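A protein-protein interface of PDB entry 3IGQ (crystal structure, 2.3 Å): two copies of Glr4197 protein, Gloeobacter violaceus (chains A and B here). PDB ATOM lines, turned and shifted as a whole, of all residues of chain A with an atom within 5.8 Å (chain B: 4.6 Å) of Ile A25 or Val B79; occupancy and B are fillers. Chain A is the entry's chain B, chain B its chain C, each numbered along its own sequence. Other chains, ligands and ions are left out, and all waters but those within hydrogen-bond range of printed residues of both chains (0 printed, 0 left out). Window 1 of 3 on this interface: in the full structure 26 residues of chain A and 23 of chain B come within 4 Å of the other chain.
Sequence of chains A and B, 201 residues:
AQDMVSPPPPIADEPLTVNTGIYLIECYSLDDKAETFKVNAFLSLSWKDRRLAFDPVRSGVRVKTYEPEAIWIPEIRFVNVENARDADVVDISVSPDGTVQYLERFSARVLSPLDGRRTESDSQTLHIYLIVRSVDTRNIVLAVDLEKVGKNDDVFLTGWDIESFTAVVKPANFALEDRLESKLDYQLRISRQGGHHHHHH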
ATOM      1  N   TYR A  23     -16.630   6.267 -14.724  1.00  0.00           N
ATOM      2  CA  TYR A  23     -16.751   7.115 -13.556  1.00  0.00           C
ATOM      3  C   TYR A  23     -15.550   6.845 -12.623  1.00  0.00           C
ATOM      4  O   TYR A  23     -15.400   5.743 -12.106  1.00  0.00           O
ATOM      5  CB  TYR A  23     -18.066   6.869 -12.849  1.00  0.00           C
ATOM      6  CG  TYR A  23     -18.318   7.890 -11.752  1.00  0.00           C
ATOM      7  CD1 TYR A  23     -17.860   7.681 -10.443  1.00  0.00           C
ATOM      8  CD2 TYR A  23     -19.019   9.071 -12.026  1.00  0.00           C
ATOM      9  CE1 TYR A  23     -18.093   8.611  -9.422  1.00  0.00           C
ATOM     10  CE2 TYR A  23     -19.268  10.019 -11.009  1.00  0.00           C
ATOM     11  CZ  TYR A  23     -18.787   9.769  -9.707  1.00  0.00           C
ATOM     12  OH  TYR A  23     -19.002  10.678  -8.702  1.00  0.00           O
ATOM     13  N   LEU A  24     -14.671   7.834 -12.453  1.00  0.00           N
ATOM     14  CA  LEU A  24     -13.435   7.580 -11.682  1.00  0.00           C
ATOM     15  C   LEU A  24     -13.731   7.550 -10.206  1.00  0.00           C
ATOM     16  O   LEU A  24     -14.365   8.480  -9.710  1.00  0.00           O
ATOM     17  CB  LEU A  24     -12.339   8.627 -11.970  1.00  0.00           C
ATOM     18  CG  LEU A  24     -11.939   8.833 -13.442  1.00  0.00           C
ATOM     19  CD1 LEU A  24     -11.071  10.057 -13.528  1.00  0.00           C
ATOM     20  CD2 LEU A  24     -11.188   7.611 -14.024  1.00  0.00           C
ATOM     21  N   ILE A  25     -13.294   6.504  -9.512  1.00  0.00           N
ATOM     22  CA  ILE A  25     -13.485   6.413  -8.087  1.00  0.00           C
ATOM     23  C   ILE A  25     -12.236   6.971  -7.382  1.00  0.00           C
ATOM     24  O   ILE A  25     -12.346   7.851  -6.539  1.00  0.00           O
ATOM     25  CB  ILE A  25     -13.752   4.954  -7.638  1.00  0.00           C
ATOM     26  CG1 ILE A  25     -15.066   4.454  -8.244  1.00  0.00           C
ATOM     27  CG2 ILE A  25     -13.853   4.907  -6.145  1.00  0.00           C
ATOM     28  CD1 ILE A  25     -15.109   2.937  -8.477  1.00  0.00           C
ATOM     29  N   GLU A  26     -11.060   6.461  -7.771  1.00  0.00           N
ATOM     30  CA  GLU A  26      -9.786   6.920  -7.233  1.00  0.00           C
ATOM     31  C   GLU A  26      -8.638   6.740  -8.234  1.00  0.00           C
ATOM     32  O   GLU A  26      -8.571   5.713  -8.901  1.00  0.00           O
ATOM     33  CB  GLU A  26      -9.423   6.154  -5.957  1.00  0.00           C
ATOM     34  CG  GLU A  26      -8.363   6.804  -5.182  1.00  0.00           C
ATOM     35  CD  GLU A  26      -8.872   8.078  -4.535  1.00  0.00           C
ATOM     36  OE1 GLU A  26      -9.954   8.016  -3.899  1.00  0.00           O
ATOM     37  OE2 GLU A  26      -8.193   9.121  -4.621  1.00  0.00           O
ATOM     38  N   CYS A  27      -7.748   7.727  -8.316  1.00  0.00           N
ATOM     39  CA  CYS A  27      -6.446   7.534  -8.914  1.00  0.00           C
ATOM     40  C   CYS A  27      -5.395   7.577  -7.809  1.00  0.00           C
ATOM     41  O   CYS A  27      -5.550   8.288  -6.795  1.00  0.00           O
ATOM     42  CB  CYS A  27      -6.194   8.587  -9.959  1.00  0.00           C
ATOM     43  SG  CYS A  27      -7.497   8.577 -11.267  1.00  0.00           S
ATOM     44  N   ASN A  40      -9.047   3.342 -10.259  1.00  0.00           N
ATOM     45  CA  ASN A  40     -10.128   2.530  -9.799  1.00  0.00           C
ATOM     46  C   ASN A  40     -11.399   3.244 -10.299  1.00  0.00           C
ATOM     47  O   ASN A  40     -11.566   4.406 -10.040  1.00  0.00           O
ATOM     48  CB  ASN A  40     -10.084   2.519  -8.271  1.00  0.00           C
ATOM     49  CG  ASN A  40     -11.110   1.564  -7.665  1.00  0.00           C
ATOM     50  OD1 ASN A  40     -12.133   2.006  -7.129  1.00  0.00           O
ATOM     51  ND2 ASN A  40     -10.839   0.257  -7.745  1.00  0.00           N
ATOM     52  N   ALA A  41     -12.261   2.558 -11.042  1.00  0.00           N
ATOM     53  CA  ALA A  41     -13.376   3.228 -11.674  1.00  0.00           C
ATOM     54  C   ALA A  41     -14.547   2.283 -12.048  1.00  0.00           C
ATOM     55  O   ALA A  41     -14.431   1.031 -11.996  1.00  0.00           O
ATOM     56  CB  ALA A  41     -12.883   3.980 -12.923  1.00  0.00           C
ATOM     57  N   PHE A  42     -15.657   2.885 -12.466  1.00  0.00           N
ATOM     58  CA  PHE A  42     -16.744   2.146 -13.056  1.00  0.00           C
ATOM     59  C   PHE A  42     -16.673   2.328 -14.553  1.00  0.00           C
ATOM     60  O   PHE A  42     -16.464   3.421 -15.045  1.00  0.00           O
ATOM     61  CB  PHE A  42     -18.103   2.699 -12.567  1.00  0.00           C
ATOM     62  CG  PHE A  42     -18.446   2.339 -11.121  1.00  0.00           C
ATOM     63  CD1 PHE A  42     -18.759   1.040 -10.746  1.00  0.00           C
ATOM     64  CD2 PHE A  42     -18.465   3.307 -10.160  1.00  0.00           C
ATOM     65  CE1 PHE A  42     -19.063   0.719  -9.438  1.00  0.00           C
ATOM     66  CE2 PHE A  42     -18.778   2.992  -8.850  1.00  0.00           C
ATOM     67  CZ  PHE A  42     -19.067   1.683  -8.501  1.00  0.00           C
ATOM     68  N   ARG A 105     -16.824  -2.633 -12.122  1.00  0.00           N
ATOM     69  CA  ARG A 105     -15.825  -1.847 -11.368  1.00  0.00           C
ATOM     70  C   ARG A 105     -14.473  -2.443 -11.777  1.00  0.00           C
ATOM     71  O   ARG A 105     -14.324  -3.664 -11.825  1.00  0.00           O
ATOM     72  CB  ARG A 105     -16.056  -2.007  -9.876  1.00  0.00           C
ATOM     73  CG  ARG A 105     -15.243  -1.073  -8.939  1.00  0.00           C
ATOM     74  CD  ARG A 105     -14.027  -1.719  -8.248  1.00  0.00           C
ATOM     75  NE  ARG A 105     -14.443  -2.539  -7.100  1.00  0.00           N
ATOM     76  CZ  ARG A 105     -14.503  -3.870  -7.103  1.00  0.00           C
ATOM     77  NH1 ARG A 105     -14.157  -4.531  -8.198  1.00  0.00           N
ATOM     78  NH2 ARG A 105     -14.904  -4.551  -6.011  1.00  0.00           N
ATOM     79  N   LYS A 151     -16.315  11.796 -12.124  1.00  0.00           N
ATOM     80  CA  LYS A 151     -15.281  11.543 -11.157  1.00  0.00           C
ATOM     81  C   LYS A 151     -15.786  11.842  -9.763  1.00  0.00           C
ATOM     82  O   LYS A 151     -16.577  12.755  -9.544  1.00  0.00           O
ATOM     83  CB  LYS A 151     -14.057  12.413 -11.473  1.00  0.00           C
ATOM     84  CG  LYS A 151     -14.414  13.871 -11.569  1.00  0.00           C
ATOM     85  CD  LYS A 151     -13.322  14.724 -12.078  1.00  0.00           C
ATOM     86  CE  LYS A 151     -13.864  16.121 -12.421  1.00  0.00           C
ATOM     87  NZ  LYS A 151     -14.425  16.809 -11.244  1.00  0.00           N
ATOM     88  N   ASN A 152     -15.294  11.069  -8.811  1.00  0.00           N
ATOM     89  CA  ASN A 152     -15.649  11.241  -7.412  1.00  0.00           C
ATOM     90  C   ASN A 152     -15.248  12.598  -6.841  1.00  0.00           C
ATOM     91  O   ASN A 152     -15.997  13.184  -6.082  1.00  0.00           O
ATOM     92  CB  ASN A 152     -15.015  10.120  -6.614  1.00  0.00           C
ATOM     93  CG  ASN A 152     -15.777   9.814  -5.385  1.00  0.00           C
ATOM     94  OD1 ASN A 152     -15.822  10.637  -4.464  1.00  0.00           O
ATOM     95  ND2 ASN A 152     -16.425   8.641  -5.356  1.00  0.00           N
ATOM     96  N   ASP A 153     -14.079  13.107  -7.198  1.00  0.00           N
ATOM     97  CA  ASP A 153     -13.684  14.452  -6.762  1.00  0.00           C
ATOM     98  C   ASP A 153     -12.713  15.206  -7.686  1.00  0.00           C
ATOM     99  O   ASP A 153     -12.516  14.826  -8.831  1.00  0.00           O
ATOM    100  CB  ASP A 153     -13.218  14.504  -5.285  1.00  0.00           C
ATOM    101  CG  ASP A 153     -11.860  13.845  -5.047  1.00  0.00           C
ATOM    102  OD1 ASP A 153     -11.241  13.231  -5.963  1.00  0.00           O
ATOM    103  OD2 ASP A 153     -11.401  13.916  -3.893  1.00  0.00           O
ATOM    104  N   ARG B  77     -19.941  -5.940  -3.085  1.00  0.00           N
ATOM    105  CA  ARG B  77     -18.687  -5.480  -3.688  1.00  0.00           C
ATOM    106  C   ARG B  77     -18.251  -4.209  -2.983  1.00  0.00           C
ATOM    107  O   ARG B  77     -19.046  -3.276  -2.856  1.00  0.00           O
ATOM    108  CB  ARG B  77     -18.897  -5.168  -5.174  1.00  0.00           C
ATOM    109  CG  ARG B  77     -19.206  -6.387  -6.044  1.00  0.00           C
ATOM    110  CD  ARG B  77     -18.145  -7.492  -5.942  1.00  0.00           C
ATOM    111  NE  ARG B  77     -18.552  -8.636  -6.768  1.00  0.00           N
ATOM    112  CZ  ARG B  77     -19.030  -9.783  -6.284  1.00  0.00           C
ATOM    113  NH1 ARG B  77     -19.141  -9.955  -4.957  1.00  0.00           N
ATOM    114  NH2 ARG B  77     -19.385 -10.771  -7.119  1.00  0.00           N
ATOM    115  N   PHE B  78     -17.030  -4.199  -2.454  1.00  0.00           N
ATOM    116  CA  PHE B  78     -16.474  -2.983  -1.949  1.00  0.00           C
ATOM    117  C   PHE B  78     -16.037  -2.111  -3.157  1.00  0.00           C
ATOM    118  O   PHE B  78     -15.344  -2.577  -4.071  1.00  0.00           O
ATOM    119  CB  PHE B  78     -15.277  -3.264  -1.049  1.00  0.00           C
ATOM    120  CG  PHE B  78     -15.613  -3.864   0.288  1.00  0.00           C
ATOM    121  CD1 PHE B  78     -16.675  -4.727   0.460  1.00  0.00           C
ATOM    122  CD2 PHE B  78     -14.812  -3.622   1.380  1.00  0.00           C
ATOM    123  CE1 PHE B  78     -16.974  -5.284   1.710  1.00  0.00           C
ATOM    124  CE2 PHE B  78     -15.123  -4.176   2.633  1.00  0.00           C
ATOM    125  CZ  PHE B  78     -16.207  -4.997   2.775  1.00  0.00           C
ATOM    126  N   VAL B  79     -16.452  -0.854  -3.193  1.00  0.00           N
ATOM    127  CA  VAL B  79     -16.133  -0.037  -4.379  1.00  0.00           C
ATOM    128  C   VAL B  79     -14.668   0.425  -4.430  1.00  0.00           C
ATOM    129  O   VAL B  79     -13.969   0.225  -5.429  1.00  0.00           O
ATOM    130  CB  VAL B  79     -17.054   1.208  -4.452  1.00  0.00           C
ATOM    131  CG1 VAL B  79     -16.712   2.031  -5.713  1.00  0.00           C
ATOM    132  CG2 VAL B  79     -18.500   0.783  -4.510  1.00  0.00           C
ATOM    133  N   ASN B  80     -14.197   1.065  -3.346  1.00  0.00           N
ATOM    134  CA  ASN B  80     -12.891   1.721  -3.378  1.00  0.00           C
ATOM    135  C   ASN B  80     -11.850   0.828  -2.692  1.00  0.00           C
ATOM    136  O   ASN B  80     -11.313   1.144  -1.635  1.00  0.00           O
ATOM    137  CB  ASN B  80     -12.975   3.072  -2.712  1.00  0.00           C
ATOM    138  CG  ASN B  80     -13.440   2.960  -1.261  1.00  0.00           C
ATOM    139  OD1 ASN B  80     -14.272   2.101  -0.934  1.00  0.00           O
ATOM    140  ND2 ASN B  80     -12.918   3.830  -0.388  1.00  0.00           N
ATOM    141  N   VAL B  81     -11.636  -0.334  -3.281  1.00  0.00           N
ATOM    142  CA  VAL B  81     -10.578  -1.205  -2.860  1.00  0.00           C
ATOM    143  C   VAL B  81      -9.704  -1.509  -4.037  1.00  0.00           C
ATOM    144  O   VAL B  81     -10.157  -1.468  -5.189  1.00  0.00           O
ATOM    145  CB  VAL B  81     -11.095  -2.541  -2.257  1.00  0.00           C
ATOM    146  CG1 VAL B  81     -11.771  -2.310  -0.929  1.00  0.00           C
ATOM    147  CG2 VAL B  81     -12.026  -3.260  -3.233  1.00  0.00           C
ATOM    148  N   TYR B 129     -16.787   2.113   0.725  1.00  0.00           N
ATOM    149  CA  TYR B 129     -18.075   2.061   0.043  1.00  0.00           C
ATOM    150  C   TYR B 129     -18.450   0.660  -0.334  1.00  0.00           C
ATOM    151  O   TYR B 129     -17.615  -0.093  -0.905  1.00  0.00           O
ATOM    152  CB  TYR B 129     -18.063   2.932  -1.206  1.00  0.00           C
ATOM    153  CG  TYR B 129     -17.832   4.425  -0.936  1.00  0.00           C
ATOM    154  CD1 TYR B 129     -18.779   5.177  -0.305  1.00  0.00           C
ATOM    155  CD2 TYR B 129     -16.640   5.063  -1.322  1.00  0.00           C
ATOM    156  CE1 TYR B 129     -18.593   6.540  -0.086  1.00  0.00           C
ATOM    157  CE2 TYR B 129     -16.431   6.439  -1.072  1.00  0.00           C
ATOM    158  CZ  TYR B 129     -17.424   7.148  -0.466  1.00  0.00           C
ATOM    159  OH  TYR B 129     -17.276   8.494  -0.238  1.00  0.00           O
ATOM    160  N   ILE B 131     -21.502  -1.710  -2.266  1.00  0.00           N
ATOM    161  CA  ILE B 131     -22.720  -1.894  -3.013  1.00  0.00           C
ATOM    162  C   ILE B 131     -23.034  -3.383  -3.055  1.00  0.00           C
ATOM    163  O   ILE B 131     -22.269  -4.173  -2.585  1.00  0.00           O
ATOM    164  CB  ILE B 131     -22.593  -1.335  -4.431  1.00  0.00           C
ATOM    165  CG1 ILE B 131     -21.552  -2.115  -5.191  1.00  0.00           C
ATOM    166  CG2 ILE B 131     -22.248   0.127  -4.418  1.00  0.00           C
ATOM    167  CD1 ILE B 131     -21.193  -1.480  -6.489  1.00  0.00           C
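ND2 of Asn A40 sits at hydrogen-bond distance from O of Val B81, at 3.2 Å. OD1 of Asn A40 lies close to O of Val B79, 3.1 Å away. NE of Arg A105 sits at hydrogen-bond distance from O of Val B79. The guanidinium group (NH2) of Arg A105 lies within hydrogen-bond range of the backbone carbonyl oxygen (O) of Phe B78.
The side-chain amide oxygen (OD1) of Asn B80 lies within hydrogen-bond range of the backbone NH (N) of Tyr B129, at 3.0 Å. N of Tyr A23 sits at hydrogen-bond distance from O of Phe A42 (2.9 Å). The backbone NH (N) of Ile A25 is in hydrogen-bond range of the backbone carbonyl oxygen (O) of Asn A40, 2.8 Å away. The backbone carbonyl oxygen of Tyr B129 sits at hydrogen-bond distance from the backbone NH of Val B79, 2.7 Å away. The backbone NH of Asn A40 sits at hydrogen-bond distance from the backbone carbonyl oxygen of Glu A26 (2.8 Å).
CD1 of Ile A25 touches CG1 of Val B79, at 3.3 Å. Ile A25 touches Asn B80. OD1 of Asn A40 touches CA of Asn B80, 3.8 Å away. Phe A42 touches Val B79 (CZ to CG1, 3.7 Å).
Of the printed residues of chain B, Ile A25 touches Val B79 (3.3 Å) and Asn B80 (3.99 Å). Val B79 touches just these residues of chain A: Ile A25, Asn A40, Phe A42 and Arg A105. Printed residues of chain A within 4 Å of Phe B78: Arg A105 (2.8 Å). Printed residues of chain B within 4 Å of Arg A105: Phe B78 and Val B79. The nearest printed residue of chain B that does not touch Ile A25 is Tyr B129 (5.6 Å). The nearest printed residue of chain B that does not touch Arg A105 is Arg B77 (4.1 Å).
Of the 12 printed residues of chain A, 4 touch a printed residue of chain B. Printed residues of chain A that touch a printed residue of chain B: Ile A25, Asn A40, Phe A42 and Arg A105. Hydrophobic or aromatic side chains of chain A within 4 Å of the printed part of chain B: Ile A25 and Phe A42. Among the printed residues, 8 pairs touch across the chains.
No position is printed for both chains. Of the 8 pairs that touch across the chains among the printed residues, none has its exchanged pair printed and touching as well.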
